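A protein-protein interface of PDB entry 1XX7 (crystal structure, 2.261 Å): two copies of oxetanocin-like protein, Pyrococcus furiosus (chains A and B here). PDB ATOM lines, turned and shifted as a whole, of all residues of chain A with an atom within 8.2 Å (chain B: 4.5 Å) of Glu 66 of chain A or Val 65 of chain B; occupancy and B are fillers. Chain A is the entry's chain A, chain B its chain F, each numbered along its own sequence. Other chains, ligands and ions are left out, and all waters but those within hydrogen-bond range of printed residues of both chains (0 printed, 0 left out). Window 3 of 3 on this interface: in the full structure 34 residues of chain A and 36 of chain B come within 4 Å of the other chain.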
ATOM      1  N   THR A  49      30.933  -4.843  37.997  1.00  0.00           N
ATOM      2  CA  THR A  49      30.941  -3.394  37.721  1.00  0.00           C
ATOM      3  C   THR A  49      29.516  -2.788  37.818  1.00  0.00           C
ATOM      4  O   THR A  49      29.312  -1.758  38.465  1.00  0.00           O
ATOM      5  CB  THR A  49      31.587  -3.076  36.322  1.00  0.00           C
ATOM      6  OG1 THR A  49      32.961  -3.462  36.313  1.00  0.00           O
ATOM      7  CG2 THR A  49      31.476  -1.590  35.985  1.00  0.00           C
ATOM      8  N   LEU A  50      28.557  -3.446  37.154  1.00  0.00           N
ATOM      9  CA  LEU A  50      27.145  -3.116  37.224  1.00  0.00           C
ATOM     10  C   LEU A  50      26.631  -3.110  38.653  1.00  0.00           C
ATOM     11  O   LEU A  50      26.033  -2.139  39.097  1.00  0.00           O
ATOM     12  CB  LEU A  50      26.350  -4.117  36.404  1.00  0.00           C
ATOM     13  CG  LEU A  50      24.826  -3.959  36.311  1.00  0.00           C
ATOM     14  CD1 LEU A  50      24.479  -2.601  35.735  1.00  0.00           C
ATOM     15  CD2 LEU A  50      24.288  -5.036  35.430  1.00  0.00           C
ATOM     16  N   ALA A  53      28.467  -0.272  40.662  1.00  0.00           N
ATOM     17  CA  ALA A  53      27.869   0.982  40.199  1.00  0.00           C
ATOM     18  C   ALA A  53      26.529   1.233  40.908  1.00  0.00           C
ATOM     19  O   ALA A  53      26.290   2.328  41.419  1.00  0.00           O
ATOM     20  CB  ALA A  53      27.677   0.962  38.682  1.00  0.00           C
ATOM     21  N   ILE A  63      28.065   7.569  38.978  1.00  0.00           N
ATOM     22  CA  ILE A  63      29.041   6.915  38.123  1.00  0.00           C
ATOM     23  C   ILE A  63      28.459   7.086  36.745  1.00  0.00           C
ATOM     24  O   ILE A  63      27.237   7.037  36.583  1.00  0.00           O
ATOM     25  CB  ILE A  63      29.176   5.410  38.523  1.00  0.00           C
ATOM     26  CG1 ILE A  63      29.845   5.276  39.907  1.00  0.00           C
ATOM     27  CG2 ILE A  63      29.920   4.574  37.459  1.00  0.00           C
ATOM     28  CD1 ILE A  63      31.348   5.673  39.979  1.00  0.00           C
ATOM     29  N   ASP A  64      29.319   7.325  35.762  1.00  0.00           N
ATOM     30  CA  ASP A  64      28.952   7.149  34.375  1.00  0.00           C
ATOM     31  C   ASP A  64      28.938   5.632  34.047  1.00  0.00           C
ATOM     32  O   ASP A  64      29.953   5.043  33.697  1.00  0.00           O
ATOM     33  CB  ASP A  64      29.957   7.905  33.515  1.00  0.00           C
ATOM     34  CG  ASP A  64      29.637   7.864  32.051  1.00  0.00           C
ATOM     35  OD1 ASP A  64      28.667   7.209  31.619  1.00  0.00           O
ATOM     36  OD2 ASP A  64      30.376   8.509  31.301  1.00  0.00           O
ATOM     37  N   VAL A  65      27.770   5.023  34.186  1.00  0.00           N
ATOM     38  CA  VAL A  65      27.615   3.598  34.092  1.00  0.00           C
ATOM     39  C   VAL A  65      27.879   3.092  32.695  1.00  0.00           C
ATOM     40  O   VAL A  65      28.526   2.068  32.535  1.00  0.00           O
ATOM     41  CB  VAL A  65      26.243   3.155  34.590  1.00  0.00           C
ATOM     42  CG1 VAL A  65      26.066   1.612  34.422  1.00  0.00           C
ATOM     43  CG2 VAL A  65      26.072   3.570  36.058  1.00  0.00           C
ATOM     44  N   GLU A  66      27.408   3.832  31.695  1.00  0.00           N
ATOM     45  CA  GLU A  66      27.689   3.530  30.321  1.00  0.00           C
ATOM     46  C   GLU A  66      29.169   3.383  30.093  1.00  0.00           C
ATOM     47  O   GLU A  66      29.611   2.327  29.581  1.00  0.00           O
ATOM     48  CB  GLU A  66      27.148   4.619  29.399  1.00  0.00           C
ATOM     49  CG  GLU A  66      27.393   4.344  27.963  1.00  0.00           C
ATOM     50  CD  GLU A  66      26.709   5.287  27.032  1.00  0.00           C
ATOM     51  OE1 GLU A  66      25.712   5.926  27.421  1.00  0.00           O
ATOM     52  OE2 GLU A  66      27.163   5.372  25.890  1.00  0.00           O
ATOM     53  N   LYS A  67      29.946   4.432  30.465  1.00  0.00           N
ATOM     54  CA  LYS A  67      31.401   4.338  30.362  1.00  0.00           C
ATOM     55  C   LYS A  67      32.035   3.173  31.150  1.00  0.00           C
ATOM     56  O   LYS A  67      32.931   2.513  30.648  1.00  0.00           O
ATOM     57  CB  LYS A  67      32.047   5.630  30.781  1.00  0.00           C
ATOM     58  CG  LYS A  67      33.598   5.596  30.766  1.00  0.00           C
ATOM     59  CD  LYS A  67      34.155   6.888  31.290  1.00  0.00           C
ATOM     60  CE  LYS A  67      34.220   7.936  30.211  1.00  0.00           C
ATOM     61  NZ  LYS A  67      34.431   9.285  30.825  1.00  0.00           N
ATOM     62  N   ALA A  68      31.580   2.934  32.362  1.00  0.00           N
ATOM     63  CA  ALA A  68      32.131   1.882  33.182  1.00  0.00           C
ATOM     64  C   ALA A  68      31.891   0.462  32.595  1.00  0.00           C
ATOM     65  O   ALA A  68      32.778  -0.387  32.656  1.00  0.00           O
ATOM     66  CB  ALA A  68      31.621   2.000  34.592  1.00  0.00           C
ATOM     67  N   LEU A  69      30.721   0.238  31.993  1.00  0.00           N
ATOM     68  CA  LEU A  69      30.426  -1.021  31.323  1.00  0.00           C
ATOM     69  C   LEU A  69      31.214  -1.161  30.042  1.00  0.00           C
ATOM     70  O   LEU A  69      31.741  -2.266  29.763  1.00  0.00           O
ATOM     71  CB  LEU A  69      28.922  -1.203  31.065  1.00  0.00           C
ATOM     72  CG  LEU A  69      28.027  -1.115  32.299  1.00  0.00           C
ATOM     73  CD1 LEU A  69      26.517  -1.181  31.893  1.00  0.00           C
ATOM     74  CD2 LEU A  69      28.383  -2.177  33.303  1.00  0.00           C
ATOM     75  N   LYS A  70      31.379  -0.089  29.268  1.00  0.00           N
ATOM     76  CA  LYS A  70      32.229  -0.219  28.071  1.00  0.00           C
ATOM     77  C   LYS A  70      33.666  -0.607  28.466  1.00  0.00           C
ATOM     78  O   LYS A  70      34.292  -1.438  27.824  1.00  0.00           O
ATOM     79  CB  LYS A  70      32.289   1.053  27.252  1.00  0.00           C
ATOM     80  CG  LYS A  70      31.045   1.474  26.528  1.00  0.00           C
ATOM     81  CD  LYS A  70      31.310   2.775  25.792  1.00  0.00           C
ATOM     82  CE  LYS A  70      30.097   3.290  25.072  1.00  0.00           C
ATOM     83  NZ  LYS A  70      30.445   4.351  24.038  1.00  0.00           N
ATOM     84  N   ILE A  71      34.171  -0.001  29.534  1.00  0.00           N
ATOM     85  CA  ILE A  71      35.546  -0.259  29.983  1.00  0.00           C
ATOM     86  C   ILE A  71      35.713  -1.712  30.428  1.00  0.00           C
ATOM     87  O   ILE A  71      36.691  -2.340  30.094  1.00  0.00           O
ATOM     88  CB  ILE A  71      35.959   0.676  31.148  1.00  0.00           C
ATOM     89  CG1 ILE A  71      36.069   2.138  30.674  1.00  0.00           C
ATOM     90  CG2 ILE A  71      37.273   0.188  31.808  1.00  0.00           C
ATOM     91  CD1 ILE A  71      36.129   3.162  31.829  1.00  0.00           C
ATOM     92  N   ALA A  72      34.749  -2.203  31.206  1.00  0.00           N
ATOM     93  CA  ALA A  72      34.745  -3.559  31.691  1.00  0.00           C
ATOM     94  C   ALA A  72      34.784  -4.605  30.544  1.00  0.00           C
ATOM     95  O   ALA A  72      35.480  -5.608  30.644  1.00  0.00           O
ATOM     96  CB  ALA A  72      33.539  -3.779  32.538  1.00  0.00           C
ATOM     97  N   ILE A  73      34.040  -4.319  29.484  1.00  0.00           N
ATOM     98  CA  ILE A  73      33.972  -5.118  28.284  1.00  0.00           C
ATOM     99  C   ILE A  73      35.266  -5.132  27.510  1.00  0.00           C
ATOM    100  O   ILE A  73      35.717  -6.211  27.085  1.00  0.00           O
ATOM    101  CB  ILE A  73      32.797  -4.690  27.374  1.00  0.00           C
ATOM    102  CG1 ILE A  73      31.486  -5.051  28.037  1.00  0.00           C
ATOM    103  CG2 ILE A  73      32.862  -5.418  26.001  1.00  0.00           C
ATOM    104  CD1 ILE A  73      30.307  -4.297  27.458  1.00  0.00           C
ATOM    105  N   TYR A 110      38.609   2.824  21.274  1.00  0.00           N
ATOM    106  CA  TYR A 110      38.526   2.521  22.706  1.00  0.00           C
ATOM    107  C   TYR A 110      39.887   2.656  23.389  1.00  0.00           C
ATOM    108  O   TYR A 110      40.153   2.006  24.417  1.00  0.00           O
ATOM    109  CB  TYR A 110      37.969   1.110  22.932  1.00  0.00           C
ATOM    110  CG  TYR A 110      36.562   0.920  22.416  1.00  0.00           C
ATOM    111  CD1 TYR A 110      35.547   1.825  22.754  1.00  0.00           C
ATOM    112  CD2 TYR A 110      36.237  -0.156  21.601  1.00  0.00           C
ATOM    113  CE1 TYR A 110      34.250   1.674  22.275  1.00  0.00           C
ATOM    114  CE2 TYR A 110      34.936  -0.325  21.132  1.00  0.00           C
ATOM    115  CZ  TYR A 110      33.950   0.602  21.476  1.00  0.00           C
ATOM    116  OH  TYR A 110      32.669   0.460  21.015  1.00  0.00           O
ATOM    117  N   LEU A 113      39.582   4.594  26.703  1.00  0.00           N
ATOM    118  CA  LEU A 113      38.884   3.740  27.684  1.00  0.00           C
ATOM    119  C   LEU A 113      39.821   2.752  28.358  1.00  0.00           C
ATOM    120  O   LEU A 113      39.757   2.593  29.580  1.00  0.00           O
ATOM    121  CB  LEU A 113      37.718   2.971  27.046  1.00  0.00           C
ATOM    122  CG  LEU A 113      36.441   3.745  26.671  1.00  0.00           C
ATOM    123  CD1 LEU A 113      35.386   2.724  26.316  1.00  0.00           C
ATOM    124  CD2 LEU A 113      35.925   4.654  27.771  1.00  0.00           C
ATOM    125  N   GLU A 124      35.408   5.872  37.092  1.00  0.00           N
ATOM    126  CA  GLU A 124      35.027   4.714  36.285  1.00  0.00           C
ATOM    127  C   GLU A 124      36.213   3.744  36.130  1.00  0.00           C
ATOM    128  O   GLU A 124      36.034   2.565  36.264  1.00  0.00           O
ATOM    129  CB  GLU A 124      34.494   5.151  34.918  1.00  0.00           C
ATOM    130  CG  GLU A 124      33.098   5.788  34.974  1.00  0.00           C
ATOM    131  CD  GLU A 124      33.090   7.230  35.599  1.00  0.00           C
ATOM    132  OE1 GLU A 124      33.972   8.028  35.269  1.00  0.00           O
ATOM    133  OE2 GLU A 124      32.226   7.512  36.461  1.00  0.00           O
ATOM    134  N   LEU B  50      27.581  -3.853  22.064  1.00  0.00           N
ATOM    135  CA  LEU B  50      28.288  -2.564  22.049  1.00  0.00           C
ATOM    136  C   LEU B  50      28.610  -2.073  20.627  1.00  0.00           C
ATOM    137  O   LEU B  50      28.409  -0.891  20.301  1.00  0.00           O
ATOM    138  CB  LEU B  50      29.575  -2.671  22.864  1.00  0.00           C
ATOM    139  CG  LEU B  50      30.538  -1.483  22.804  1.00  0.00           C
ATOM    140  CD1 LEU B  50      29.824  -0.226  23.334  1.00  0.00           C
ATOM    141  CD2 LEU B  50      31.712  -1.805  23.639  1.00  0.00           C
ATOM    142  N   ALA B  53      25.214  -1.244  18.906  1.00  0.00           N
ATOM    143  CA  ALA B  53      24.690   0.017  19.448  1.00  0.00           C
ATOM    144  C   ALA B  53      25.424   1.227  18.902  1.00  0.00           C
ATOM    145  O   ALA B  53      24.785   2.217  18.586  1.00  0.00           O
ATOM    146  CB  ALA B  53      24.712   0.032  20.962  1.00  0.00           C
ATOM    147  N   GLU B  54      26.753   1.142  18.800  1.00  0.00           N
ATOM    148  CA  GLU B  54      27.567   2.237  18.264  1.00  0.00           C
ATOM    149  C   GLU B  54      27.350   2.408  16.757  1.00  0.00           C
ATOM    150  O   GLU B  54      27.379   3.512  16.255  1.00  0.00           O
ATOM    151  CB  GLU B  54      29.082   2.063  18.574  1.00  0.00           C
ATOM    152  CG  GLU B  54      29.458   2.209  20.068  1.00  0.00           C
ATOM    153  CD  GLU B  54      28.961   3.528  20.707  1.00  0.00           C
ATOM    154  OE1 GLU B  54      28.841   4.557  19.997  1.00  0.00           O
ATOM    155  OE2 GLU B  54      28.716   3.537  21.939  1.00  0.00           O
ATOM    156  N   ILE B  63      19.299   5.560  20.576  1.00  0.00           N
ATOM    157  CA  ILE B  63      19.601   4.268  21.198  1.00  0.00           C
ATOM    158  C   ILE B  63      20.154   4.561  22.588  1.00  0.00           C
ATOM    159  O   ILE B  63      21.018   5.415  22.740  1.00  0.00           O
ATOM    160  CB  ILE B  63      20.627   3.435  20.340  1.00  0.00           C
ATOM    161  CG1 ILE B  63      20.934   2.058  20.968  1.00  0.00           C
ATOM    162  CG2 ILE B  63      21.926   4.191  20.127  1.00  0.00           C
ATOM    163  CD1 ILE B  63      20.009   0.959  20.489  1.00  0.00           C
ATOM    164  N   ASP B  64      19.631   3.874  23.591  1.00  0.00           N
ATOM    165  CA  ASP B  64      20.182   3.928  24.956  1.00  0.00           C
ATOM    166  C   ASP B  64      21.248   2.818  25.115  1.00  0.00           C
ATOM    167  O   ASP B  64      20.903   1.647  25.356  1.00  0.00           O
ATOM    168  CB  ASP B  64      19.065   3.743  25.962  1.00  0.00           C
ATOM    169  CG  ASP B  64      19.490   4.020  27.353  1.00  0.00           C
ATOM    170  OD1 ASP B  64      20.697   4.047  27.628  1.00  0.00           O
ATOM    171  OD2 ASP B  64      18.598   4.193  28.199  1.00  0.00           O
ATOM    172  N   VAL B  65      22.521   3.210  24.968  1.00  0.00           N
ATOM    173  CA  VAL B  65      23.646   2.282  24.941  1.00  0.00           C
ATOM    174  C   VAL B  65      23.838   1.620  26.296  1.00  0.00           C
ATOM    175  O   VAL B  65      23.908   0.388  26.392  1.00  0.00           O
ATOM    176  CB  VAL B  65      24.958   2.959  24.447  1.00  0.00           C
ATOM    177  CG1 VAL B  65      26.139   1.959  24.487  1.00  0.00           C
ATOM    178  CG2 VAL B  65      24.787   3.486  23.005  1.00  0.00           C
ATOM    179  N   GLU B  66      23.912   2.436  27.338  1.00  0.00           N
ATOM    180  CA  GLU B  66      23.948   1.952  28.704  1.00  0.00           C
ATOM    181  C   GLU B  66      22.914   0.844  28.959  1.00  0.00           C
ATOM    182  O   GLU B  66      23.260  -0.181  29.518  1.00  0.00           O
ATOM    183  CB  GLU B  66      23.698   3.083  29.703  1.00  0.00           C
ATOM    184  CG  GLU B  66      23.643   2.571  31.135  1.00  0.00           C
ATOM    185  CD  GLU B  66      23.398   3.668  32.146  1.00  0.00           C
ATOM    186  OE1 GLU B  66      23.629   4.829  31.804  1.00  0.00           O
ATOM    187  OE2 GLU B  66      22.978   3.358  33.282  1.00  0.00           O
ATOM    188  N   LYS B  67      21.644   1.083  28.591  1.00  0.00           N
ATOM    189  CA  LYS B  67      20.583   0.089  28.795  1.00  0.00           C
ATOM    190  C   LYS B  67      20.794  -1.227  28.060  1.00  0.00           C
ATOM    191  O   LYS B  67      20.613  -2.272  28.635  1.00  0.00           O
ATOM    192  CB  LYS B  67      19.240   0.621  28.357  1.00  0.00           C
ATOM    193  CG  LYS B  67      18.083  -0.218  28.896  1.00  0.00           C
ATOM    194  CD  LYS B  67      16.740   0.396  28.522  1.00  0.00           C
ATOM    195  CE  LYS B  67      15.801   0.359  29.682  1.00  0.00           C
ATOM    196  NZ  LYS B  67      14.414   0.337  29.157  1.00  0.00           N
ATOM    197  N   ALA B  68      21.114  -1.145  26.778  1.00  0.00           N
ATOM    198  CA  ALA B  68      21.389  -2.322  25.964  1.00  0.00           C
ATOM    199  C   ALA B  68      22.543  -3.191  26.565  1.00  0.00           C
ATOM    200  O   ALA B  68      22.472  -4.426  26.564  1.00  0.00           O
ATOM    201  CB  ALA B  68      21.730  -1.897  24.584  1.00  0.00           C
ATOM    202  N   LEU B  69      23.587  -2.520  27.060  1.00  0.00           N
ATOM    203  CA  LEU B  69      24.685  -3.199  27.721  1.00  0.00           C
ATOM    204  C   LEU B  69      24.253  -3.884  29.008  1.00  0.00           C
ATOM    205  O   LEU B  69      24.656  -5.004  29.252  1.00  0.00           O
ATOM    206  CB  LEU B  69      25.886  -2.253  27.990  1.00  0.00           C
ATOM    207  CG  LEU B  69      26.599  -1.642  26.775  1.00  0.00           C
ATOM    208  CD1 LEU B  69      27.740  -0.705  27.200  1.00  0.00           C
ATOM    209  CD2 LEU B  69      27.085  -2.693  25.808  1.00  0.00           C
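The side-chain carboxylate (OE2) of Glu 54 of chain B is in salt-bridge range of the side-chain amino group (NZ) of Lys 70 of chain A (2.8 Å).
The side-chain carboxylate (OE2) of Glu 66 of chain A lies within salt-bridge range of the side-chain amino group (NZ) of Lys 70 of chain A (3.9 Å).
Of chain B, only Val 65 and Glu 66 come within 4 Å of Glu 66 of chain A. Of the printed residues of chain B, Lys 70 of chain A touches Leu 50 and Glu 54. Of the printed residues of chain B, Ile 73 of chain A touches Leu 69 (3.96 Å). Of chain A, only Glu 66 comes within 4 Å of Val 65 of chain B. Of the printed residues of chain A, Glu 66 of chain B touches Val 65 and Glu 66. Of the printed residues of chain A, Leu 69 of chain B touches Ile 73 (3.96 Å). The nearest printed residue of chain B that does not touch Val 65 of chain A is Leu 69 of chain B (6.1 Å).
Among the printed residues, pairs that only touch across the chains: Val 65 of chain A with Glu 66 of chain B, Glu 66 of chain A with Val 65 of chain B, Glu 66 of chain A with Glu 66 of chain B, Lys 70 of chain A with Leu 50 of chain B, Ile 73 of chain A with Leu 69 of chain B, Tyr 110 of chain A with Leu 50 of chain B and Tyr 110 of chain A with Glu 54 of chain B.
Val 65 of chain A touches Glu 66 of chain B, and with the chains exchanged Glu 66 of chain A touches Val 65 of chain B. Glu 66 of chain A touches its own counterpart, Glu 66 of chain B. Positions printed for both chains: 50, 53, 63, 64, 65, 66, 67, 68 and 69. Of the 8 pairs that touch across the chains among the printed residues, 3 have their exchanged pair printed and touching as well.
Of the 10 printed residues of chain B, 5 touch a printed residue of chain A. Hydrophobic or aromatic side chains of chain B within 4 Å of the printed part of chain A: Leu 50, Val 65 and Leu 69. Printed residues of chain A that touch a printed residue of chain B: Val 65, Glu 66, Lys 70, Ile 73 and Tyr 110. Among the printed residues, 8 pairs touch across the chains.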
